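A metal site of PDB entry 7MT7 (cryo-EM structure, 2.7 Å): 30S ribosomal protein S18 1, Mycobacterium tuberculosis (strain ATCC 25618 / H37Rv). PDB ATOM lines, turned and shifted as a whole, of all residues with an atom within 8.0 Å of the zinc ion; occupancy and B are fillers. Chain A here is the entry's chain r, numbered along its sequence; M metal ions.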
ATOM      1  N   LYS A  19      -8.821  27.230  14.558  1.00  0.00           N
ATOM      2  CA  LYS A  19      -8.789  28.054  15.755  1.00  0.00           C
ATOM      3  C   LYS A  19      -9.430  27.248  16.873  1.00  0.00           C
ATOM      4  O   LYS A  19      -9.039  27.358  18.029  1.00  0.00           O
ATOM      5  CB  LYS A  19      -9.523  29.372  15.525  1.00  0.00           C
ATOM      6  CG  LYS A  19      -9.120  30.500  16.481  1.00  0.00           C
ATOM      7  CD  LYS A  19      -9.994  30.611  17.705  1.00  0.00           C
ATOM      8  CE  LYS A  19      -9.617  31.854  18.477  1.00  0.00           C
ATOM      9  NZ  LYS A  19      -8.222  31.792  18.991  1.00  0.00           N
ATOM     10  N   CYS A  20     -10.394  26.416  16.494  1.00  0.00           N
ATOM     11  CA  CYS A  20     -11.010  25.466  17.418  1.00  0.00           C
ATOM     12  C   CYS A  20     -10.248  24.151  17.347  1.00  0.00           C
ATOM     13  O   CYS A  20     -10.006  23.621  16.259  1.00  0.00           O
ATOM     14  CB  CYS A  20     -12.483  25.245  17.085  1.00  0.00           C
ATOM     15  SG  CYS A  20     -13.338  24.119  18.220  1.00  0.00           S
ATOM     16  N   VAL A  21      -9.890  23.629  18.520  1.00  0.00           N
ATOM     17  CA  VAL A  21      -9.061  22.429  18.592  1.00  0.00           C
ATOM     18  C   VAL A  21      -9.852  21.202  18.138  1.00  0.00           C
ATOM     19  O   VAL A  21      -9.337  20.362  17.391  1.00  0.00           O
ATOM     20  CB  VAL A  21      -8.518  22.274  20.014  1.00  0.00           C
ATOM     21  CG1 VAL A  21      -7.775  20.972  20.185  1.00  0.00           C
ATOM     22  CG2 VAL A  21      -7.625  23.457  20.356  1.00  0.00           C
ATOM     23  N   PHE A  22     -11.114  21.119  18.546  1.00  0.00           N
ATOM     24  CA  PHE A  22     -11.909  19.933  18.257  1.00  0.00           C
ATOM     25  C   PHE A  22     -12.390  19.906  16.819  1.00  0.00           C
ATOM     26  O   PHE A  22     -12.665  18.839  16.282  1.00  0.00           O
ATOM     27  CB  PHE A  22     -13.105  19.879  19.208  1.00  0.00           C
ATOM     28  CG  PHE A  22     -12.707  19.827  20.649  1.00  0.00           C
ATOM     29  CD1 PHE A  22     -12.286  18.638  21.227  1.00  0.00           C
ATOM     30  CD2 PHE A  22     -12.742  20.963  21.424  1.00  0.00           C
ATOM     31  CE1 PHE A  22     -11.924  18.597  22.553  1.00  0.00           C
ATOM     32  CE2 PHE A  22     -12.381  20.930  22.743  1.00  0.00           C
ATOM     33  CZ  PHE A  22     -11.967  19.742  23.308  1.00  0.00           C
ATOM     34  N   CYS A  23     -12.493  21.072  16.187  1.00  0.00           N
ATOM     35  CA  CYS A  23     -12.858  21.101  14.775  1.00  0.00           C
ATOM     36  C   CYS A  23     -11.663  20.811  13.881  1.00  0.00           C
ATOM     37  O   CYS A  23     -11.821  20.203  12.823  1.00  0.00           O
ATOM     38  CB  CYS A  23     -13.477  22.443  14.416  1.00  0.00           C
ATOM     39  SG  CYS A  23     -15.083  22.757  15.173  1.00  0.00           S
ATOM     40  N   ALA A  24     -10.470  21.245  14.289  1.00  0.00           N
ATOM     41  CA  ALA A  24      -9.276  20.978  13.509  1.00  0.00           C
ATOM     42  C   ALA A  24      -8.886  19.503  13.614  1.00  0.00           C
ATOM     43  O   ALA A  24      -8.860  18.784  12.611  1.00  0.00           O
ATOM     44  CB  ALA A  24      -8.123  21.876  13.955  1.00  0.00           C
ATOM     45  N   LYS A  25      -8.605  19.044  14.824  1.00  0.00           N
ATOM     46  CA  LYS A  25      -8.318  17.643  15.044  1.00  0.00           C
ATOM     47  C   LYS A  25      -9.652  16.909  15.080  1.00  0.00           C
ATOM     48  O   LYS A  25     -10.407  17.021  16.044  1.00  0.00           O
ATOM     49  CB  LYS A  25      -7.530  17.460  16.346  1.00  0.00           C
ATOM     50  CG  LYS A  25      -6.838  16.106  16.498  1.00  0.00           C
ATOM     51  CD  LYS A  25      -7.639  15.098  17.289  1.00  0.00           C
ATOM     52  CE  LYS A  25      -6.832  13.817  17.501  1.00  0.00           C
ATOM     53  NZ  LYS A  25      -7.568  12.789  18.272  1.00  0.00           N
ATOM     54  N   ILE A  30     -14.863  13.884  23.196  1.00  0.00           N
ATOM     55  CA  ILE A  30     -15.106  14.706  24.367  1.00  0.00           C
ATOM     56  C   ILE A  30     -15.867  13.840  25.365  1.00  0.00           C
ATOM     57  O   ILE A  30     -17.044  13.509  25.142  1.00  0.00           O
ATOM     58  CB  ILE A  30     -15.875  15.975  24.015  1.00  0.00           C
ATOM     59  CG1 ILE A  30     -15.059  16.820  23.044  1.00  0.00           C
ATOM     60  CG2 ILE A  30     -16.163  16.743  25.269  1.00  0.00           C
ATOM     61  CD1 ILE A  30     -15.870  17.922  22.411  1.00  0.00           C
ATOM     62  N   GLY A  55     -11.596  29.511  22.293  1.00  0.00           N
ATOM     63  CA  GLY A  55     -11.664  29.413  20.852  1.00  0.00           C
ATOM     64  C   GLY A  55     -12.571  28.326  20.319  1.00  0.00           C
ATOM     65  O   GLY A  55     -12.472  27.996  19.130  1.00  0.00           O
ATOM     66  N   ASN A  56     -13.434  27.753  21.148  1.00  0.00           N
ATOM     67  CA  ASN A  56     -14.294  26.686  20.688  1.00  0.00           C
ATOM     68  C   ASN A  56     -15.444  27.233  19.852  1.00  0.00           C
ATOM     69  O   ASN A  56     -15.818  28.398  19.942  1.00  0.00           O
ATOM     70  CB  ASN A  56     -14.873  25.902  21.863  1.00  0.00           C
ATOM     71  CG  ASN A  56     -13.848  25.059  22.560  1.00  0.00           C
ATOM     72  OD1 ASN A  56     -12.991  24.443  21.937  1.00  0.00           O
ATOM     73  ND2 ASN A  56     -13.948  24.999  23.874  1.00  0.00           N
ATOM     74  N   CYS A  57     -16.034  26.347  19.062  1.00  0.00           N
ATOM     75  CA  CYS A  57     -17.268  26.654  18.368  1.00  0.00           C
ATOM     76  C   CYS A  57     -18.426  26.584  19.354  1.00  0.00           C
ATOM     77  O   CYS A  57     -18.255  26.332  20.542  1.00  0.00           O
ATOM     78  CB  CYS A  57     -17.463  25.716  17.179  1.00  0.00           C
ATOM     79  SG  CYS A  57     -17.698  23.987  17.598  1.00  0.00           S
ATOM     80  N   VAL A  58     -19.638  26.815  18.856  1.00  0.00           N
ATOM     81  CA  VAL A  58     -20.808  26.719  19.727  1.00  0.00           C
ATOM     82  C   VAL A  58     -21.065  25.267  20.110  1.00  0.00           C
ATOM     83  O   VAL A  58     -21.382  24.965  21.258  1.00  0.00           O
ATOM     84  CB  VAL A  58     -22.032  27.356  19.049  1.00  0.00           C
ATOM     85  CG1 VAL A  58     -23.236  27.271  19.937  1.00  0.00           C
ATOM     86  CG2 VAL A  58     -21.757  28.782  18.693  1.00  0.00           C
ATOM     87  N   GLN A  59     -20.872  24.355  19.163  1.00  0.00           N
ATOM     88  CA  GLN A  59     -21.292  22.978  19.374  1.00  0.00           C
ATOM     89  C   GLN A  59     -20.329  22.217  20.278  1.00  0.00           C
ATOM     90  O   GLN A  59     -20.764  21.319  21.002  1.00  0.00           O
ATOM     91  CB  GLN A  59     -21.411  22.252  18.046  1.00  0.00           C
ATOM     92  CG  GLN A  59     -22.359  22.887  17.091  1.00  0.00           C
ATOM     93  CD  GLN A  59     -22.539  22.082  15.851  1.00  0.00           C
ATOM     94  OE1 GLN A  59     -22.004  20.986  15.732  1.00  0.00           O
ATOM     95  NE2 GLN A  59     -23.272  22.616  14.896  1.00  0.00           N
ATOM     96  N   HIS A  60     -19.050  22.554  20.250  1.00  0.00           N
ATOM     97  CA  HIS A  60     -18.116  21.866  21.121  1.00  0.00           C
ATOM     98  C   HIS A  60     -18.060  22.495  22.504  1.00  0.00           C
ATOM     99  O   HIS A  60     -17.781  21.785  23.469  1.00  0.00           O
ATOM    100  CB  HIS A  60     -16.734  21.811  20.494  1.00  0.00           C
ATOM    101  CG  HIS A  60     -16.655  20.925  19.298  1.00  0.00           C
ATOM    102  ND1 HIS A  60     -16.719  21.396  18.002  1.00  0.00           N
ATOM    103  CD2 HIS A  60     -16.585  19.576  19.196  1.00  0.00           C
ATOM    104  CE1 HIS A  60     -16.642  20.384  17.161  1.00  0.00           C
ATOM    105  NE2 HIS A  60     -16.559  19.272  17.856  1.00  0.00           N
ATOM    106  N   GLN A  61     -18.330  23.793  22.616  1.00  0.00           N
ATOM    107  CA  GLN A  61     -18.504  24.405  23.933  1.00  0.00           C
ATOM    108  C   GLN A  61     -19.701  23.805  24.644  1.00  0.00           C
ATOM    109  O   GLN A  61     -19.698  23.657  25.873  1.00  0.00           O
ATOM    110  CB  GLN A  61     -18.678  25.916  23.768  1.00  0.00           C
ATOM    111  CG  GLN A  61     -18.798  26.702  25.056  1.00  0.00           C
ATOM    112  CD  GLN A  61     -17.521  26.749  25.833  1.00  0.00           C
ATOM    113  OE1 GLN A  61     -16.442  26.832  25.262  1.00  0.00           O
ATOM    114  NE2 GLN A  61     -17.632  26.729  27.147  1.00  0.00           N
ATOM    115  N   ASP A  63     -20.521  20.653  24.102  1.00  0.00           N
ATOM    116  CA  ASP A  63     -20.059  19.304  24.437  1.00  0.00           C
ATOM    117  C   ASP A  63     -19.029  19.304  25.551  1.00  0.00           C
ATOM    118  O   ASP A  63     -18.902  18.306  26.257  1.00  0.00           O
ATOM    119  CB  ASP A  63     -19.496  18.627  23.202  1.00  0.00           C
ATOM    120  CG  ASP A  63     -20.576  18.221  22.220  1.00  0.00           C
ATOM    121  OD1 ASP A  63     -21.701  17.937  22.653  1.00  0.00           O
ATOM    122  OD2 ASP A  63     -20.287  18.194  21.001  1.00  0.00           O
HETATM  123 ZN    ZN M   1     -15.414  23.031  17.584  1.00  0.00          ZN
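The side-chain sulfur (SG) of Cys 20 lies close to the backbone NH (N) of Phe 22.
SG of Cys 20 lies close to OD1 of Asn 56, 3.7 Å away.
N of Gln 59 sits close to SG of Cys 57, at 3.6 Å.
Of the 16 residues printed, 4 come within 4 Å of the zinc ion.
The zinc ion is bound by ND1 of His 60 (2.1 Å), SG of Cys 20 (2.4 Å), SG of Cys 23 (2.4 Å) and SG of Cys 57 (2.5 Å).
The zinc ion has four donor atoms within binding distance.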
